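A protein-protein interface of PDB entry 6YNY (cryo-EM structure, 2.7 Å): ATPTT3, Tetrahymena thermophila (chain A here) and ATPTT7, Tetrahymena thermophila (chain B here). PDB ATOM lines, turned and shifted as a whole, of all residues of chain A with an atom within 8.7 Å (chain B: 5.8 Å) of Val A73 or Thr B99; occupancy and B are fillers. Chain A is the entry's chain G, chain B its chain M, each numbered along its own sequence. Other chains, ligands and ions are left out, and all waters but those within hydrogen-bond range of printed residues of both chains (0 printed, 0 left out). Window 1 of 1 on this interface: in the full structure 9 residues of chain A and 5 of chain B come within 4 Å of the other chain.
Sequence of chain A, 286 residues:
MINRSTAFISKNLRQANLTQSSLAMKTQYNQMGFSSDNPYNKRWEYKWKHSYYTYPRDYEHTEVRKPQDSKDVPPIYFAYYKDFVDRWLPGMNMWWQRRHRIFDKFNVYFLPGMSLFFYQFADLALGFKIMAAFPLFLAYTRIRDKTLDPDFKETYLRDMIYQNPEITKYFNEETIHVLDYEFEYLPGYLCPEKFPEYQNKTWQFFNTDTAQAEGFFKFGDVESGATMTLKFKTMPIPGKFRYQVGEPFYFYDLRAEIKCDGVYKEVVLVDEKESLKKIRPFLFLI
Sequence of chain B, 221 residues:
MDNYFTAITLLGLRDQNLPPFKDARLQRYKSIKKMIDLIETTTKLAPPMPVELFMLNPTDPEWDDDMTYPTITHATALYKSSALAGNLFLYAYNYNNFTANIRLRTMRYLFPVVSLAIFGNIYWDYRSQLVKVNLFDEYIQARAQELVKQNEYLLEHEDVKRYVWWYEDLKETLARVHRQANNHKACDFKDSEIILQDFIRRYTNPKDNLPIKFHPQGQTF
NH1 of Arg B108 lies within hydrogen-bond range of O of Pro A74, at 2.8 Å.
O of Tyr B95 sits at hydrogen-bond distance from OG1 of Thr B99.
The backbone carbonyl oxygen of Thr B99 is in hydrogen-bond range of the guanidinium group of Arg B108 (3.4 Å).
Thr B99 touches Val A73 (CG2 to CG1, 3.7 Å).
Ala B100 touches Val A73 (CB to CG1, 3.9 Å).
NH2 of Arg B108 touches O of Val A73, at 3.9 Å.
NH1 of Arg B108 touches O of Pro A75, 3.8 Å away.
Ile A76 touches Arg B108 (CD1 to O, 3.2 Å).
Thr B99 touches just one residue of chain A: Val A73.
Printed residues of chain B within 4 Å of Pro A74: Arg B108.
Of the printed residues of chain A, Arg B108 touches Val A73 (3.9 Å), Pro A74 (2.8 Å), Pro A75 (3.8 Å) and Ile A76 (3.2 Å).
Of the printed residues of chain B, Pro A75 touches Arg B108.
Printed residues of chain B within 4 Å of Ile A76: Arg B108 (3.2 Å).
Arg A57 touches none of the printed residues of chain B.
Of the 10 printed residues of chain A, 4 touch a printed residue of chain B.
Printed residues of chain B that touch a printed residue of chain A: Thr B99, Ala B100 and Arg B108.
Among the printed residues, no Asp or Glu carboxylate lies within 4 Å of a Lys or Arg side-chain nitrogen of the other chain.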
ATOM      1  N   ARG A  57       0.841   8.562   4.036  1.00  0.00           N
ATOM      2  CA  ARG A  57       0.270   7.320   4.542  1.00  0.00           C
ATOM      3  C   ARG A  57      -0.983   7.585   5.361  1.00  0.00           C
ATOM      4  O   ARG A  57      -2.032   6.972   5.135  1.00  0.00           O
ATOM      5  CB  ARG A  57       1.306   6.583   5.384  1.00  0.00           C
ATOM      6  CG  ARG A  57       0.876   5.209   5.840  1.00  0.00           C
ATOM      7  CD  ARG A  57       1.849   4.648   6.840  1.00  0.00           C
ATOM      8  NE  ARG A  57       1.869   5.436   8.062  1.00  0.00           N
ATOM      9  CZ  ARG A  57       2.729   5.251   9.053  1.00  0.00           C
ATOM     10  NH1 ARG A  57       2.672   6.018  10.129  1.00  0.00           N
ATOM     11  NH2 ARG A  57       3.645   4.303   8.971  1.00  0.00           N
ATOM     12  N   ASP A  58      -0.889   8.496   6.321  1.00  0.00           N
ATOM     13  CA  ASP A  58      -1.997   8.838   7.194  1.00  0.00           C
ATOM     14  C   ASP A  58      -2.310  10.318   7.061  1.00  0.00           C
ATOM     15  O   ASP A  58      -1.439  11.126   6.729  1.00  0.00           O
ATOM     16  CB  ASP A  58      -1.669   8.512   8.654  1.00  0.00           C
ATOM     17  CG  ASP A  58      -1.115   7.115   8.831  1.00  0.00           C
ATOM     18  OD1 ASP A  58      -1.512   6.212   8.066  1.00  0.00           O
ATOM     19  OD2 ASP A  58      -0.277   6.919   9.734  1.00  0.00           O
ATOM     20  N   SER A  70      -0.916   3.520  13.809  1.00  0.00           N
ATOM     21  CA  SER A  70      -0.890   3.516  12.357  1.00  0.00           C
ATOM     22  C   SER A  70      -0.566   2.119  11.842  1.00  0.00           C
ATOM     23  O   SER A  70      -0.222   1.209  12.599  1.00  0.00           O
ATOM     24  CB  SER A  70       0.125   4.532  11.829  1.00  0.00           C
ATOM     25  OG  SER A  70       1.413   4.276  12.348  1.00  0.00           O
ATOM     26  N   LYS A  71      -0.678   1.961  10.529  1.00  0.00           N
ATOM     27  CA  LYS A  71      -0.487   0.680   9.862  1.00  0.00           C
ATOM     28  C   LYS A  71       0.765   0.754   8.999  1.00  0.00           C
ATOM     29  O   LYS A  71       0.783   1.451   7.980  1.00  0.00           O
ATOM     30  CB  LYS A  71      -1.717   0.333   9.027  1.00  0.00           C
ATOM     31  CG  LYS A  71      -1.609  -0.950   8.242  1.00  0.00           C
ATOM     32  CD  LYS A  71      -2.970  -1.408   7.742  1.00  0.00           C
ATOM     33  CE  LYS A  71      -3.675  -0.327   6.942  1.00  0.00           C
ATOM     34  NZ  LYS A  71      -4.940  -0.820   6.326  1.00  0.00           N
ATOM     35  N   ASP A  72       1.806   0.034   9.409  1.00  0.00           N
ATOM     36  CA  ASP A  72       3.018  -0.047   8.612  1.00  0.00           C
ATOM     37  C   ASP A  72       2.724  -0.712   7.273  1.00  0.00           C
ATOM     38  O   ASP A  72       1.746  -1.448   7.117  1.00  0.00           O
ATOM     39  CB  ASP A  72       4.092  -0.834   9.357  1.00  0.00           C
ATOM     40  CG  ASP A  72       4.414  -0.243  10.713  1.00  0.00           C
ATOM     41  OD1 ASP A  72       4.343   0.995  10.859  1.00  0.00           O
ATOM     42  OD2 ASP A  72       4.739  -1.019  11.637  1.00  0.00           O
ATOM     43  N   VAL A  73       3.591  -0.443   6.301  1.00  0.00           N
ATOM     44  CA  VAL A  73       3.537  -1.076   4.982  1.00  0.00           C
ATOM     45  C   VAL A  73       2.088  -1.133   4.518  1.00  0.00           C
ATOM     46  O   VAL A  73       1.497  -2.220   4.469  1.00  0.00           O
ATOM     47  CB  VAL A  73       4.187  -2.469   4.972  1.00  0.00           C
ATOM     48  CG1 VAL A  73       5.693  -2.330   4.987  1.00  0.00           C
ATOM     49  CG2 VAL A  73       3.709  -3.329   6.130  1.00  0.00           C
ATOM     50  N   PRO A  74       1.479   0.002   4.194  1.00  0.00           N
ATOM     51  CA  PRO A  74       0.052   0.020   3.896  1.00  0.00           C
ATOM     52  C   PRO A  74      -0.306  -0.997   2.832  1.00  0.00           C
ATOM     53  O   PRO A  74       0.573  -1.512   2.125  1.00  0.00           O
ATOM     54  CB  PRO A  74      -0.188   1.450   3.396  1.00  0.00           C
ATOM     55  CG  PRO A  74       1.139   1.955   3.011  1.00  0.00           C
ATOM     56  CD  PRO A  74       2.117   1.292   3.902  1.00  0.00           C
ATOM     57  N   PRO A  75      -1.588  -1.309   2.685  1.00  0.00           N
ATOM     58  CA  PRO A  75      -1.987  -2.388   1.781  1.00  0.00           C
ATOM     59  C   PRO A  75      -1.567  -2.104   0.351  1.00  0.00           C
ATOM     60  O   PRO A  75      -1.139  -1.007  -0.012  1.00  0.00           O
ATOM     61  CB  PRO A  75      -3.509  -2.424   1.926  1.00  0.00           C
ATOM     62  CG  PRO A  75      -3.869  -1.065   2.385  1.00  0.00           C
ATOM     63  CD  PRO A  75      -2.753  -0.626   3.265  1.00  0.00           C
ATOM     64  N   ILE A  76      -1.693  -3.138  -0.475  1.00  0.00           N
ATOM     65  CA  ILE A  76      -1.343  -3.014  -1.877  1.00  0.00           C
ATOM     66  C   ILE A  76      -2.424  -2.219  -2.602  1.00  0.00           C
ATOM     67  O   ILE A  76      -3.616  -2.310  -2.287  1.00  0.00           O
ATOM     68  CB  ILE A  76      -1.143  -4.410  -2.493  1.00  0.00           C
ATOM     69  CG1 ILE A  76      -0.607  -4.294  -3.914  1.00  0.00           C
ATOM     70  CG2 ILE A  76      -2.436  -5.202  -2.466  1.00  0.00           C
ATOM     71  CD1 ILE A  76      -0.269  -5.612  -4.536  1.00  0.00           C
ATOM     72  N   PHE A  78      -2.570   1.039  -2.474  1.00  0.00           N
ATOM     73  CA  PHE A  78      -2.965   2.092  -1.548  1.00  0.00           C
ATOM     74  C   PHE A  78      -2.862   3.471  -2.186  1.00  0.00           C
ATOM     75  O   PHE A  78      -3.689   4.346  -1.913  1.00  0.00           O
ATOM     76  CB  PHE A  78      -2.099   2.013  -0.296  1.00  0.00           C
ATOM     77  CG  PHE A  78      -2.294   3.148   0.658  1.00  0.00           C
ATOM     78  CD1 PHE A  78      -3.392   3.190   1.492  1.00  0.00           C
ATOM     79  CD2 PHE A  78      -1.366   4.167   0.735  1.00  0.00           C
ATOM     80  CE1 PHE A  78      -3.564   4.227   2.369  1.00  0.00           C
ATOM     81  CE2 PHE A  78      -1.536   5.205   1.613  1.00  0.00           C
ATOM     82  CZ  PHE A  78      -2.635   5.235   2.431  1.00  0.00           C
ATOM     83  N   TYR B  91      11.652 -11.026  -5.835  1.00  0.00           N
ATOM     84  CA  TYR B  91      10.759 -10.229  -5.006  1.00  0.00           C
ATOM     85  C   TYR B  91      10.896 -10.604  -3.539  1.00  0.00           C
ATOM     86  O   TYR B  91      10.919  -9.730  -2.668  1.00  0.00           O
ATOM     87  CB  TYR B  91       9.316 -10.404  -5.468  1.00  0.00           C
ATOM     88  CG  TYR B  91       8.393  -9.326  -4.966  1.00  0.00           C
ATOM     89  CD1 TYR B  91       8.036  -8.263  -5.776  1.00  0.00           C
ATOM     90  CD2 TYR B  91       7.892  -9.359  -3.677  1.00  0.00           C
ATOM     91  CE1 TYR B  91       7.205  -7.275  -5.321  1.00  0.00           C
ATOM     92  CE2 TYR B  91       7.062  -8.375  -3.215  1.00  0.00           C
ATOM     93  CZ  TYR B  91       6.721  -7.334  -4.039  1.00  0.00           C
ATOM     94  OH  TYR B  91       5.889  -6.349  -3.575  1.00  0.00           O
ATOM     95  N   ASN B  94      14.052  -9.315  -2.042  1.00  0.00           N
ATOM     96  CA  ASN B  94      13.969  -7.870  -1.891  1.00  0.00           C
ATOM     97  C   ASN B  94      12.599  -7.449  -1.371  1.00  0.00           C
ATOM     98  O   ASN B  94      12.071  -6.402  -1.746  1.00  0.00           O
ATOM     99  CB  ASN B  94      14.256  -7.168  -3.213  1.00  0.00           C
ATOM    100  CG  ASN B  94      15.524  -7.643  -3.874  1.00  0.00           C
ATOM    101  OD1 ASN B  94      15.490  -8.266  -4.931  1.00  0.00           O
ATOM    102  ND2 ASN B  94      16.655  -7.334  -3.265  1.00  0.00           N
ATOM    103  N   TYR B  95      12.013  -8.254  -0.485  1.00  0.00           N
ATOM    104  CA  TYR B  95      10.641  -8.004  -0.052  1.00  0.00           C
ATOM    105  C   TYR B  95      10.524  -6.690   0.707  1.00  0.00           C
ATOM    106  O   TYR B  95       9.598  -5.906   0.473  1.00  0.00           O
ATOM    107  CB  TYR B  95      10.150  -9.163   0.812  1.00  0.00           C
ATOM    108  CG  TYR B  95       8.738  -8.988   1.306  1.00  0.00           C
ATOM    109  CD1 TYR B  95       7.659  -9.261   0.485  1.00  0.00           C
ATOM    110  CD2 TYR B  95       8.484  -8.543   2.591  1.00  0.00           C
ATOM    111  CE1 TYR B  95       6.375  -9.098   0.928  1.00  0.00           C
ATOM    112  CE2 TYR B  95       7.201  -8.377   3.041  1.00  0.00           C
ATOM    113  CZ  TYR B  95       6.148  -8.655   2.206  1.00  0.00           C
ATOM    114  OH  TYR B  95       4.861  -8.491   2.652  1.00  0.00           O
ATOM    115  N   ASN B  96      11.450  -6.432   1.628  1.00  0.00           N
ATOM    116  CA  ASN B  96      11.344  -5.240   2.457  1.00  0.00           C
ATOM    117  C   ASN B  96      11.421  -3.968   1.628  1.00  0.00           C
ATOM    118  O   ASN B  96      10.782  -2.967   1.968  1.00  0.00           O
ATOM    119  CB  ASN B  96      12.440  -5.245   3.517  1.00  0.00           C
ATOM    120  CG  ASN B  96      13.824  -5.222   2.922  1.00  0.00           C
ATOM    121  OD1 ASN B  96      14.116  -5.932   1.962  1.00  0.00           O
ATOM    122  ND2 ASN B  96      14.688  -4.393   3.485  1.00  0.00           N
ATOM    123  N   ASN B  97      12.188  -3.985   0.542  1.00  0.00           N
ATOM    124  CA  ASN B  97      12.325  -2.799  -0.290  1.00  0.00           C
ATOM    125  C   ASN B  97      11.091  -2.584  -1.160  1.00  0.00           C
ATOM    126  O   ASN B  97      10.561  -1.471  -1.233  1.00  0.00           O
ATOM    127  CB  ASN B  97      13.572  -2.921  -1.159  1.00  0.00           C
ATOM    128  CG  ASN B  97      14.844  -2.996  -0.355  1.00  0.00           C
ATOM    129  OD1 ASN B  97      15.316  -4.079  -0.015  1.00  0.00           O
ATOM    130  ND2 ASN B  97      15.415  -1.846  -0.054  1.00  0.00           N
ATOM    131  N   PHE B  98      10.624  -3.640  -1.826  1.00  0.00           N
ATOM    132  CA  PHE B  98       9.438  -3.527  -2.666  1.00  0.00           C
ATOM    133  C   PHE B  98       8.194  -3.188  -1.860  1.00  0.00           C
ATOM    134  O   PHE B  98       7.273  -2.549  -2.380  1.00  0.00           O
ATOM    135  CB  PHE B  98       9.211  -4.829  -3.430  1.00  0.00           C
ATOM    136  CG  PHE B  98      10.157  -5.044  -4.566  1.00  0.00           C
ATOM    137  CD1 PHE B  98      10.404  -4.046  -5.483  1.00  0.00           C
ATOM    138  CD2 PHE B  98      10.796  -6.253  -4.719  1.00  0.00           C
ATOM    139  CE1 PHE B  98      11.270  -4.252  -6.523  1.00  0.00           C
ATOM    140  CE2 PHE B  98      11.663  -6.461  -5.760  1.00  0.00           C
ATOM    141  CZ  PHE B  98      11.899  -5.459  -6.662  1.00  0.00           C
ATOM    142  N   THR B  99       8.147  -3.596  -0.597  1.00  0.00           N
ATOM    143  CA  THR B  99       6.948  -3.440   0.213  1.00  0.00           C
ATOM    144  C   THR B  99       6.912  -2.128   0.984  1.00  0.00           C
ATOM    145  O   THR B  99       5.848  -1.513   1.099  1.00  0.00           O
ATOM    146  CB  THR B  99       6.828  -4.612   1.187  1.00  0.00           C
ATOM    147  OG1 THR B  99       6.864  -5.844   0.460  1.00  0.00           O
ATOM    148  CG2 THR B  99       5.547  -4.537   1.959  1.00  0.00           C
ATOM    149  N   ALA B 100       8.044  -1.682   1.516  1.00  0.00           N
ATOM    150  CA  ALA B 100       8.072  -0.505   2.374  1.00  0.00           C
ATOM    151  C   ALA B 100       8.538   0.757   1.669  1.00  0.00           C
ATOM    152  O   ALA B 100       8.146   1.854   2.075  1.00  0.00           O
ATOM    153  CB  ALA B 100       8.971  -0.762   3.583  1.00  0.00           C
ATOM    154  N   ASN B 101       9.364   0.639   0.636  1.00  0.00           N
ATOM    155  CA  ASN B 101       9.835   1.807  -0.095  1.00  0.00           C
ATOM    156  C   ASN B 101       8.800   2.198  -1.140  1.00  0.00           C
ATOM    157  O   ASN B 101       8.462   1.399  -2.018  1.00  0.00           O
ATOM    158  CB  ASN B 101      11.183   1.520  -0.746  1.00  0.00           C
ATOM    159  CG  ASN B 101      11.862   2.769  -1.248  1.00  0.00           C
ATOM    160  OD1 ASN B 101      11.219   3.673  -1.776  1.00  0.00           O
ATOM    161  ND2 ASN B 101      13.171   2.830  -1.079  1.00  0.00           N
ATOM    162  N   ARG B 108       5.432  -3.265  -6.725  1.00  0.00           N
ATOM    163  CA  ARG B 108       4.615  -3.989  -5.763  1.00  0.00           C
ATOM    164  C   ARG B 108       3.192  -4.168  -6.266  1.00  0.00           C
ATOM    165  O   ARG B 108       2.565  -5.198  -5.999  1.00  0.00           O
ATOM    166  CB  ARG B 108       4.614  -3.251  -4.428  1.00  0.00           C
ATOM    167  CG  ARG B 108       3.806  -3.922  -3.339  1.00  0.00           C
ATOM    168  CD  ARG B 108       3.641  -3.029  -2.138  1.00  0.00           C
ATOM    169  NE  ARG B 108       2.950  -3.704  -1.049  1.00  0.00           N
ATOM    170  CZ  ARG B 108       2.466  -3.088   0.021  1.00  0.00           C
ATOM    171  NH1 ARG B 108       2.590  -1.778   0.150  1.00  0.00           N
ATOM    172  NH2 ARG B 108       1.854  -3.784   0.961  1.00  0.00           N
